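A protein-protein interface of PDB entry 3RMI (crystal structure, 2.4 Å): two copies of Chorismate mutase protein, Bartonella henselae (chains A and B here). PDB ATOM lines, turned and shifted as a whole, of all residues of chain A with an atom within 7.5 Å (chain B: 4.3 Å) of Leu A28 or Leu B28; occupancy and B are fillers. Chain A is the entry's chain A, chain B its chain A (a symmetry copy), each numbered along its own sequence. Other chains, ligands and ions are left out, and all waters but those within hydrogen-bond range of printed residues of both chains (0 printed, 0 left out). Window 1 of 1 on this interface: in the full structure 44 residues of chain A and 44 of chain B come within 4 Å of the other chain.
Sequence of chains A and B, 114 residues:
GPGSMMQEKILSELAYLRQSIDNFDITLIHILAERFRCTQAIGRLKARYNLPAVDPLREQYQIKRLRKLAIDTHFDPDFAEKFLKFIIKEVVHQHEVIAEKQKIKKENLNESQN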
ATOM      1  N   ILE A  21      11.504  10.525  19.556  1.00  0.00           N
ATOM      2  CA  ILE A  21      10.224  10.503  18.871  1.00  0.00           C
ATOM      3  C   ILE A  21       9.184  11.155  19.735  1.00  0.00           C
ATOM      4  O   ILE A  21       8.452  12.033  19.298  1.00  0.00           O
ATOM      5  CB  ILE A  21       9.841   9.065  18.523  1.00  0.00           C
ATOM      6  CG1 ILE A  21      10.760   8.572  17.395  1.00  0.00           C
ATOM      7  CG2 ILE A  21       8.359   8.975  18.113  1.00  0.00           C
ATOM      8  CD1 ILE A  21      10.914   7.066  17.403  1.00  0.00           C
ATOM      9  N   ASP A  22       9.125  10.728  20.984  1.00  0.00           N
ATOM     10  CA  ASP A  22       8.106  11.225  21.913  1.00  0.00           C
ATOM     11  C   ASP A  22       8.214  12.745  22.114  1.00  0.00           C
ATOM     12  O   ASP A  22       7.209  13.448  22.187  1.00  0.00           O
ATOM     13  CB  ASP A  22       8.220  10.480  23.227  1.00  0.00           C
ATOM     14  CG  ASP A  22       7.656   9.037  23.146  1.00  0.00           C
ATOM     15  OD1 ASP A  22       7.060   8.679  22.087  1.00  0.00           O
ATOM     16  OD2 ASP A  22       7.770   8.284  24.157  1.00  0.00           O
ATOM     17  N   ASN A  23       9.447  13.247  22.114  1.00  0.00           N
ATOM     18  CA  ASN A  23       9.700  14.668  22.173  1.00  0.00           C
ATOM     19  C   ASN A  23       9.294  15.401  20.908  1.00  0.00           C
ATOM     20  O   ASN A  23       8.809  16.551  20.944  1.00  0.00           O
ATOM     21  CB  ASN A  23      11.186  14.863  22.328  1.00  0.00           C
ATOM     22  CG  ASN A  23      11.518  15.885  23.348  1.00  0.00           C
ATOM     23  OD1 ASN A  23      11.506  15.592  24.577  1.00  0.00           O
ATOM     24  ND2 ASN A  23      11.861  17.091  22.879  1.00  0.00           N
ATOM     25  N   PHE A  24       9.574  14.774  19.764  1.00  0.00           N
ATOM     26  CA  PHE A  24       9.157  15.384  18.502  1.00  0.00           C
ATOM     27  C   PHE A  24       7.640  15.508  18.461  1.00  0.00           C
ATOM     28  O   PHE A  24       7.119  16.528  18.045  1.00  0.00           O
ATOM     29  CB  PHE A  24       9.658  14.596  17.317  1.00  0.00           C
ATOM     30  CG  PHE A  24      11.159  14.617  17.164  1.00  0.00           C
ATOM     31  CD1 PHE A  24      11.866  15.781  17.317  1.00  0.00           C
ATOM     32  CD2 PHE A  24      11.852  13.456  16.856  1.00  0.00           C
ATOM     33  CE1 PHE A  24      13.233  15.790  17.173  1.00  0.00           C
ATOM     34  CE2 PHE A  24      13.205  13.456  16.694  1.00  0.00           C
ATOM     35  CZ  PHE A  24      13.905  14.606  16.860  1.00  0.00           C
ATOM     36  N   ASP A  25       6.946  14.480  18.918  1.00  0.00           N
ATOM     37  CA  ASP A  25       5.493  14.493  18.900  1.00  0.00           C
ATOM     38  C   ASP A  25       4.893  15.603  19.772  1.00  0.00           C
ATOM     39  O   ASP A  25       3.897  16.193  19.378  1.00  0.00           O
ATOM     40  CB  ASP A  25       4.941  13.124  19.290  1.00  0.00           C
ATOM     41  CG  ASP A  25       5.136  12.056  18.168  1.00  0.00           C
ATOM     42  OD1 ASP A  25       5.416  12.440  17.006  1.00  0.00           O
ATOM     43  OD2 ASP A  25       5.028  10.821  18.449  1.00  0.00           O
ATOM     44  N   ILE A  26       5.484  15.914  20.926  1.00  0.00           N
ATOM     45  CA  ILE A  26       4.971  17.035  21.729  1.00  0.00           C
ATOM     46  C   ILE A  26       5.168  18.334  21.005  1.00  0.00           C
ATOM     47  O   ILE A  26       4.333  19.221  21.077  1.00  0.00           O
ATOM     48  CB  ILE A  26       5.673  17.320  23.064  1.00  0.00           C
ATOM     49  CG1 ILE A  26       6.051  16.084  23.794  1.00  0.00           C
ATOM     50  CG2 ILE A  26       4.710  18.137  23.973  1.00  0.00           C
ATOM     51  CD1 ILE A  26       6.381  16.327  25.307  1.00  0.00           C
ATOM     52  N   THR A  27       6.343  18.475  20.424  1.00  0.00           N
ATOM     53  CA  THR A  27       6.707  19.647  19.630  1.00  0.00           C
ATOM     54  C   THR A  27       5.751  19.845  18.485  1.00  0.00           C
ATOM     55  O   THR A  27       5.271  20.948  18.249  1.00  0.00           O
ATOM     56  CB  THR A  27       8.127  19.465  19.103  1.00  0.00           C
ATOM     57  OG1 THR A  27       8.975  19.090  20.219  1.00  0.00           O
ATOM     58  CG2 THR A  27       8.636  20.725  18.524  1.00  0.00           C
ATOM     59  N   LEU A  28       5.447  18.761  17.780  1.00  0.00           N
ATOM     60  CA  LEU A  28       4.523  18.837  16.662  1.00  0.00           C
ATOM     61  C   LEU A  28       3.152  19.306  17.110  1.00  0.00           C
ATOM     62  O   LEU A  28       2.513  20.097  16.418  1.00  0.00           O
ATOM     63  CB  LEU A  28       4.418  17.484  15.948  1.00  0.00           C
ATOM     64  CG  LEU A  28       5.643  17.026  15.135  1.00  0.00           C
ATOM     65  CD1 LEU A  28       5.454  15.567  14.746  1.00  0.00           C
ATOM     66  CD2 LEU A  28       5.849  17.877  13.884  1.00  0.00           C
ATOM     67  N   ILE A  29       2.697  18.836  18.267  1.00  0.00           N
ATOM     68  CA  ILE A  29       1.398  19.267  18.788  1.00  0.00           C
ATOM     69  C   ILE A  29       1.417  20.750  19.184  1.00  0.00           C
ATOM     70  O   ILE A  29       0.439  21.466  18.977  1.00  0.00           O
ATOM     71  CB  ILE A  29       0.970  18.430  20.017  1.00  0.00           C
ATOM     72  CG1 ILE A  29       0.562  17.017  19.565  1.00  0.00           C
ATOM     73  CG2 ILE A  29      -0.218  19.083  20.786  1.00  0.00           C
ATOM     74  CD1 ILE A  29      -0.600  16.984  18.540  1.00  0.00           C
ATOM     75  N   HIS A  30       2.501  21.216  19.792  1.00  0.00           N
ATOM     76  CA  HIS A  30       2.548  22.652  20.146  1.00  0.00           C
ATOM     77  C   HIS A  30       2.543  23.559  18.915  1.00  0.00           C
ATOM     78  O   HIS A  30       1.827  24.538  18.901  1.00  0.00           O
ATOM     79  CB  HIS A  30       3.730  22.964  21.041  1.00  0.00           C
ATOM     80  CG  HIS A  30       3.501  22.598  22.466  1.00  0.00           C
ATOM     81  ND1 HIS A  30       4.165  21.563  23.082  1.00  0.00           N
ATOM     82  CD2 HIS A  30       2.669  23.121  23.397  1.00  0.00           C
ATOM     83  CE1 HIS A  30       3.782  21.486  24.344  1.00  0.00           C
ATOM     84  NE2 HIS A  30       2.875  22.420  24.561  1.00  0.00           N
ATOM     85  N   ILE A  31       3.249  23.175  17.859  1.00  0.00           N
ATOM     86  CA  ILE A  31       3.234  23.941  16.619  1.00  0.00           C
ATOM     87  C   ILE A  31       1.899  23.910  15.918  1.00  0.00           C
ATOM     88  O   ILE A  31       1.402  24.939  15.455  1.00  0.00           O
ATOM     89  CB  ILE A  31       4.296  23.434  15.646  1.00  0.00           C
ATOM     90  CG1 ILE A  31       5.665  23.806  16.194  1.00  0.00           C
ATOM     91  CG2 ILE A  31       4.131  24.079  14.274  1.00  0.00           C
ATOM     92  CD1 ILE A  31       6.777  22.938  15.577  1.00  0.00           C
ATOM     93  N   LEU A  32       1.298  22.734  15.837  1.00  0.00           N
ATOM     94  CA  LEU A  32      -0.070  22.637  15.330  1.00  0.00           C
ATOM     95  C   LEU A  32      -1.107  23.414  16.166  1.00  0.00           C
ATOM     96  O   LEU A  32      -2.042  23.993  15.598  1.00  0.00           O
ATOM     97  CB  LEU A  32      -0.497  21.196  15.249  1.00  0.00           C
ATOM     98  CG  LEU A  32       0.067  20.319  14.147  1.00  0.00           C
ATOM     99  CD1 LEU A  32      -0.434  18.874  14.462  1.00  0.00           C
ATOM    100  CD2 LEU A  32      -0.427  20.769  12.806  1.00  0.00           C
ATOM    101  N   ALA A  33      -0.958  23.437  17.487  1.00  0.00           N
ATOM    102  CA  ALA A  33      -1.803  24.304  18.291  1.00  0.00           C
ATOM    103  C   ALA A  33      -1.748  25.729  17.771  1.00  0.00           C
ATOM    104  O   ALA A  33      -2.778  26.372  17.640  1.00  0.00           O
ATOM    105  CB  ALA A  33      -1.400  24.294  19.764  1.00  0.00           C
ATOM    106  N   GLU A  34      -0.551  26.251  17.509  1.00  0.00           N
ATOM    107  CA  GLU A  34      -0.478  27.622  16.998  1.00  0.00           C
ATOM    108  C   GLU A  34      -1.051  27.738  15.586  1.00  0.00           C
ATOM    109  O   GLU A  34      -1.722  28.718  15.281  1.00  0.00           O
ATOM    110  CB  GLU A  34       0.941  28.179  17.046  1.00  0.00           C
ATOM    111  CG  GLU A  34       1.411  28.527  18.458  1.00  0.00           C
ATOM    112  CD  GLU A  34       0.500  29.535  19.171  1.00  0.00           C
ATOM    113  OE1 GLU A  34       0.189  30.626  18.609  1.00  0.00           O
ATOM    114  OE2 GLU A  34       0.098  29.222  20.307  1.00  0.00           O
ATOM    115  N   ARG A  35      -0.804  26.740  14.746  1.00  0.00           N
ATOM    116  CA  ARG A  35      -1.305  26.761  13.361  1.00  0.00           C
ATOM    117  C   ARG A  35      -2.815  26.834  13.360  1.00  0.00           C
ATOM    118  O   ARG A  35      -3.405  27.573  12.553  1.00  0.00           O
ATOM    119  CB  ARG A  35      -0.909  25.497  12.627  1.00  0.00           C
ATOM    120  CG  ARG A  35      -1.021  25.606  11.088  1.00  0.00           C
ATOM    121  CD  ARG A  35      -0.925  24.244  10.480  1.00  0.00           C
ATOM    122  NE  ARG A  35      -0.805  24.239   9.028  1.00  0.00           N
ATOM    123  CZ  ARG A  35      -1.823  24.432   8.180  1.00  0.00           C
ATOM    124  NH1 ARG A  35      -3.043  24.723   8.614  1.00  0.00           N
ATOM    125  NH2 ARG A  35      -1.612  24.360   6.890  1.00  0.00           N
ATOM    126  N   LEU A  66       5.209  23.417  -0.388  1.00  0.00           N
ATOM    127  CA  LEU A  66       5.679  22.461   0.591  1.00  0.00           C
ATOM    128  C   LEU A  66       6.407  21.305  -0.091  1.00  0.00           C
ATOM    129  O   LEU A  66       7.382  20.772   0.432  1.00  0.00           O
ATOM    130  CB  LEU A  66       4.531  21.967   1.480  1.00  0.00           C
ATOM    131  CG  LEU A  66       4.992  21.473   2.857  1.00  0.00           C
ATOM    132  CD1 LEU A  66       5.642  22.640   3.650  1.00  0.00           C
ATOM    133  CD2 LEU A  66       3.839  20.857   3.644  1.00  0.00           C
ATOM    134  N   PHE A  75      13.218  15.254   2.017  1.00  0.00           N
ATOM    135  CA  PHE A  75      11.987  14.712   2.584  1.00  0.00           C
ATOM    136  C   PHE A  75      11.002  14.386   1.447  1.00  0.00           C
ATOM    137  O   PHE A  75      10.892  15.164   0.478  1.00  0.00           O
ATOM    138  CB  PHE A  75      11.386  15.777   3.494  1.00  0.00           C
ATOM    139  CG  PHE A  75      10.274  15.289   4.361  1.00  0.00           C
ATOM    140  CD1 PHE A  75      10.524  14.868   5.645  1.00  0.00           C
ATOM    141  CD2 PHE A  75       8.971  15.263   3.898  1.00  0.00           C
ATOM    142  CE1 PHE A  75       9.485  14.425   6.458  1.00  0.00           C
ATOM    143  CE2 PHE A  75       7.940  14.835   4.706  1.00  0.00           C
ATOM    144  CZ  PHE A  75       8.196  14.418   5.990  1.00  0.00           C
ATOM    145  N   PHE A  83       0.438  14.826   4.087  1.00  0.00           N
ATOM    146  CA  PHE A  83       0.379  15.437   5.419  1.00  0.00           C
ATOM    147  C   PHE A  83      -0.342  16.781   5.401  1.00  0.00           C
ATOM    148  O   PHE A  83      -1.234  17.038   6.219  1.00  0.00           O
ATOM    149  CB  PHE A  83       1.783  15.590   5.989  1.00  0.00           C
ATOM    150  CG  PHE A  83       1.852  16.479   7.203  1.00  0.00           C
ATOM    151  CD1 PHE A  83       1.289  16.106   8.376  1.00  0.00           C
ATOM    152  CD2 PHE A  83       2.472  17.712   7.143  1.00  0.00           C
ATOM    153  CE1 PHE A  83       1.341  16.946   9.483  1.00  0.00           C
ATOM    154  CE2 PHE A  83       2.526  18.531   8.242  1.00  0.00           C
ATOM    155  CZ  PHE A  83       1.957  18.135   9.408  1.00  0.00           C
ATOM    156  N   LEU A  84       0.026  17.645   4.468  1.00  0.00           N
ATOM    157  CA  LEU A  84      -0.643  18.928   4.365  1.00  0.00           C
ATOM    158  C   LEU A  84      -2.138  18.763   4.059  1.00  0.00           C
ATOM    159  O   LEU A  84      -2.981  19.454   4.637  1.00  0.00           O
ATOM    160  CB  LEU A  84       0.034  19.777   3.305  1.00  0.00           C
ATOM    161  CG  LEU A  84      -0.519  21.172   3.022  1.00  0.00           C
ATOM    162  CD1 LEU A  84      -0.446  22.097   4.236  1.00  0.00           C
ATOM    163  CD2 LEU A  84       0.250  21.756   1.833  1.00  0.00           C
ATOM    164  N   ILE A  87      -3.988  17.959   7.138  1.00  0.00           N
ATOM    165  CA  ILE A  87      -4.237  19.141   7.943  1.00  0.00           C
ATOM    166  C   ILE A  87      -5.347  20.007   7.318  1.00  0.00           C
ATOM    167  O   ILE A  87      -6.250  20.482   8.011  1.00  0.00           O
ATOM    168  CB  ILE A  87      -2.972  19.976   8.121  1.00  0.00           C
ATOM    169  CG1 ILE A  87      -1.898  19.171   8.856  1.00  0.00           C
ATOM    170  CG2 ILE A  87      -3.273  21.206   8.914  1.00  0.00           C
ATOM    171  CD1 ILE A  87      -2.337  18.747  10.265  1.00  0.00           C
ATOM    172  N   PHE B  24       4.708  27.770   9.925  1.00  0.00           N
ATOM    173  CA  PHE B  24       4.473  26.605  10.775  1.00  0.00           C
ATOM    174  C   PHE B  24       4.635  25.327   9.962  1.00  0.00           C
ATOM    175  O   PHE B  24       5.237  24.376  10.430  1.00  0.00           O
ATOM    176  CB  PHE B  24       3.106  26.657  11.416  1.00  0.00           C
ATOM    177  CG  PHE B  24       2.947  27.777  12.413  1.00  0.00           C
ATOM    178  CD1 PHE B  24       3.931  28.053  13.326  1.00  0.00           C
ATOM    179  CD2 PHE B  24       1.792  28.544  12.430  1.00  0.00           C
ATOM    180  CE1 PHE B  24       3.773  29.075  14.233  1.00  0.00           C
ATOM    181  CE2 PHE B  24       1.617  29.549  13.334  1.00  0.00           C
ATOM    182  CZ  PHE B  24       2.599  29.830  14.229  1.00  0.00           C
ATOM    183  N   ASP B  25       4.121  25.327   8.744  1.00  0.00           N
ATOM    184  CA  ASP B  25       4.205  24.147   7.899  1.00  0.00           C
ATOM    185  C   ASP B  25       5.649  23.756   7.559  1.00  0.00           C
ATOM    186  O   ASP B  25       5.946  22.571   7.512  1.00  0.00           O
ATOM    187  CB  ASP B  25       3.371  24.336   6.634  1.00  0.00           C
ATOM    188  CG  ASP B  25       1.836  24.263   6.911  1.00  0.00           C
ATOM    189  OD1 ASP B  25       1.438  23.778   8.000  1.00  0.00           O
ATOM    190  OD2 ASP B  25       1.019  24.710   6.048  1.00  0.00           O
ATOM    191  N   ILE B  26       6.549  24.715   7.346  1.00  0.00           N
ATOM    192  CA  ILE B  26       7.955  24.355   7.105  1.00  0.00           C
ATOM    193  C   ILE B  26       8.556  23.735   8.331  1.00  0.00           C
ATOM    194  O   ILE B  26       9.359  22.821   8.240  1.00  0.00           O
ATOM    195  CB  ILE B  26       8.937  25.503   6.831  1.00  0.00           C
ATOM    196  CG1 ILE B  26       8.356  26.568   5.973  1.00  0.00           C
ATOM    197  CG2 ILE B  26      10.187  24.931   6.104  1.00  0.00           C
ATOM    198  CD1 ILE B  26       9.431  27.521   5.346  1.00  0.00           C
ATOM    199  N   THR B  27       8.257  24.340   9.465  1.00  0.00           N
ATOM    200  CA  THR B  27       8.705  23.860  10.770  1.00  0.00           C
ATOM    201  C   THR B  27       8.239  22.450  11.019  1.00  0.00           C
ATOM    202  O   THR B  27       9.011  21.596  11.439  1.00  0.00           O
ATOM    203  CB  THR B  27       8.163  24.790  11.852  1.00  0.00           C
ATOM    204  OG1 THR B  27       8.477  26.154  11.467  1.00  0.00           O
ATOM    205  CG2 THR B  27       8.801  24.506  13.153  1.00  0.00           C
ATOM    206  N   LEU B  28       6.968  22.193  10.731  1.00  0.00           N
ATOM    207  CA  LEU B  28       6.418  20.861  10.921  1.00  0.00           C
ATOM    208  C   LEU B  28       7.139  19.840  10.063  1.00  0.00           C
ATOM    209  O   LEU B  28       7.401  18.727  10.516  1.00  0.00           O
ATOM    210  CB  LEU B  28       4.915  20.845  10.620  1.00  0.00           C
ATOM    211  CG  LEU B  28       3.993  21.562  11.624  1.00  0.00           C
ATOM    212  CD1 LEU B  28       2.603  21.675  11.018  1.00  0.00           C
ATOM    213  CD2 LEU B  28       3.921  20.824  12.961  1.00  0.00           C
ATOM    214  N   ILE B  29       7.475  20.208   8.831  1.00  0.00           N
ATOM    215  CA  ILE B  29       8.206  19.293   7.951  1.00  0.00           C
ATOM    216  C   ILE B  29       9.630  19.039   8.465  1.00  0.00           C
ATOM    217  O   ILE B  29      10.139  17.924   8.377  1.00  0.00           O
ATOM    218  CB  ILE B  29       8.289  19.836   6.506  1.00  0.00           C
ATOM    219  CG1 ILE B  29       6.910  19.727   5.831  1.00  0.00           C
ATOM    220  CG2 ILE B  29       9.339  19.066   5.649  1.00  0.00           C
ATOM    221  CD1 ILE B  29       6.343  18.287   5.765  1.00  0.00           C
ATOM    222  N   HIS B  30      10.302  20.069   8.964  1.00  0.00           N
ATOM    223  CA  HIS B  30      11.662  19.831   9.498  1.00  0.00           C
ATOM    224  C   HIS B  30      11.660  18.918  10.723  1.00  0.00           C
ATOM    225  O   HIS B  30      12.478  18.027  10.802  1.00  0.00           O
ATOM    226  CB  HIS B  30      12.376  21.134   9.796  1.00  0.00           C
ATOM    227  CG  HIS B  30      12.942  21.787   8.584  1.00  0.00           C
ATOM    228  ND1 HIS B  30      12.438  22.958   8.070  1.00  0.00           N
ATOM    229  CD2 HIS B  30      13.962  21.425   7.773  1.00  0.00           C
ATOM    230  CE1 HIS B  30      13.150  23.315   7.014  1.00  0.00           C
ATOM    231  NE2 HIS B  30      14.080  22.401   6.813  1.00  0.00           N
ATOM    232  N   ILE B  31      10.683  19.072  11.609  1.00  0.00           N
ATOM    233  CA  ILE B  31      10.563  18.191  12.764  1.00  0.00           C
ATOM    234  C   ILE B  31      10.199  16.774  12.393  1.00  0.00           C
ATOM    235  O   ILE B  31      10.778  15.815  12.908  1.00  0.00           O
ATOM    236  CB  ILE B  31       9.516  18.710  13.745  1.00  0.00           C
ATOM    237  CG1 ILE B  31      10.060  19.968  14.405  1.00  0.00           C
ATOM    238  CG2 ILE B  31       9.228  17.680  14.833  1.00  0.00           C
ATOM    239  CD1 ILE B  31       8.934  20.823  15.013  1.00  0.00           C
ATOM    240  N   LEU B  32       9.241  16.623  11.492  1.00  0.00           N
ATOM    241  CA  LEU B  32       8.941  15.299  10.948  1.00  0.00           C
ATOM    242  C   LEU B  32      10.121  14.643  10.202  1.00  0.00           C
ATOM    243  O   LEU B  32      10.303  13.423  10.294  1.00  0.00           O
ATOM    244  CB  LEU B  32       7.761  15.371  10.015  1.00  0.00           C
ATOM    245  CG  LEU B  32       6.371  15.545  10.596  1.00  0.00           C
ATOM    246  CD1 LEU B  32       5.428  15.760   9.370  1.00  0.00           C
ATOM    247  CD2 LEU B  32       5.964  14.327  11.369  1.00  0.00           C
ATOM    248  N   PHE B  83      -4.034  12.493  14.332  1.00  0.00           N
ATOM    249  CA  PHE B  83      -2.749  12.926  13.772  1.00  0.00           C
ATOM    250  C   PHE B  83      -1.639  11.913  14.036  1.00  0.00           C
ATOM    251  O   PHE B  83      -0.896  11.530  13.124  1.00  0.00           O
ATOM    252  CB  PHE B  83      -2.369  14.292  14.327  1.00  0.00           C
ATOM    253  CG  PHE B  83      -0.938  14.681  14.058  1.00  0.00           C
ATOM    254  CD1 PHE B  83      -0.508  14.940  12.801  1.00  0.00           C
ATOM    255  CD2 PHE B  83      -0.020  14.758  15.088  1.00  0.00           C
ATOM    256  CE1 PHE B  83       0.821  15.276  12.566  1.00  0.00           C
ATOM    257  CE2 PHE B  83       1.287  15.098  14.846  1.00  0.00           C
ATOM    258  CZ  PHE B  83       1.694  15.356  13.580  1.00  0.00           C
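NE of Arg A35 is in salt-bridge range of OD1 of Asp B25, 2.5 Å away.
The backbone carbonyl oxygen (O) of Asn A23 is in hydrogen-bond range of the side-chain hydroxyl (OG1) of Thr A27 (2.6 Å).
Among the printed residues, pairs that only touch across the chains: Ile A31 with Ile B31 (3.1 Å), Leu A84 with Asp B25 (3.5 Å), Leu A28 with Ile B31 (3.5 Å), Ile A31 with Leu B28 (3.5 Å), Thr A27 with Ile B31 (3.5 Å), Ile A31 with Thr B27 (3.5 Å), Phe A83 with Phe B83 (3.5 Å), Leu A32 with Leu B28 (3.6 Å), Leu A28 with Leu B32 (3.6 Å), Leu A28 with Leu B28 (3.6 Å), Glu A34 with Phe B24 (3.7 Å), Arg A35 with Phe B24 (3.7 Å), Phe A75 with Leu B32 (3.8 Å), Leu A66 with Ile B29 (3.9 Å), Leu A66 with Asp B25 (3.9 Å), Phe A83 with Leu B28 (3.9 Å), Leu A28 with Phe B83 (3.9 Å), Phe A75 with Ile B29 (3.9 Å), Ile A31 with Phe B24 (3.98 Å) and Phe A24 with Ile B31 (3.98 Å).
Leu A28 touches four residues of chain B.
Of chain A, only Leu A28 (3.6 Å), Ile A31 (3.5 Å), Leu A32 (3.6 Å) and Phe A83 (3.9 Å) come within 4 Å of Leu B28.
Of the printed residues of chain A, Thr B27 touches Ile A31.
Of the printed residues of chain B, Arg A35 touches Phe B24 (3.7 Å) and Asp B25 (2.5 Å).
Printed residues of chain A within 4 Å of Asp B25: Arg A35, Leu A66 and Leu A84.
Of the printed residues of chain B, Phe A83 touches Leu B28 and Phe B83.
Of the printed residues of chain A, Phe B24 touches Ile A31, Glu A34 and Arg A35.
Ile A21 touches none of the printed residues of chain B.
Asp A25 touches none of the printed residues of chain B.
The nearest printed residue of chain B that does not touch Leu A28 is Thr B27 (5.5 Å).
The nearest residue of chain A that does not touch Leu B28 is Arg A35 (4.4 Å).
Of the 20 printed residues of chain A, 11 touch a printed residue of chain B.
Hydrophobic or aromatic side chains of chain A that line the printed part of chain B: Phe A24, Leu A28, Ile A31, Leu A32, Leu A66, Phe A75, Phe A83 and Leu A84.
Of the 10 printed residues of chain B, 8 touch a printed residue of chain A.
Among the printed residues, 21 pairs touch across the chains.
Phe A24 touches Ile B31, and with the chains exchanged Ile A31 touches Phe B24.
Thr A27 touches Ile B31, and with the chains exchanged Ile A31 touches Thr B27.
Leu A28 touches Phe B83, and with the chains exchanged Phe A83 touches Leu B28.
Ile B31 touches its own counterpart, Ile A31.
10 positions are printed for both chains.
Of the 21 pairs that touch across the chains among the printed residues, 13 have their exchanged pair printed and touching as well.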
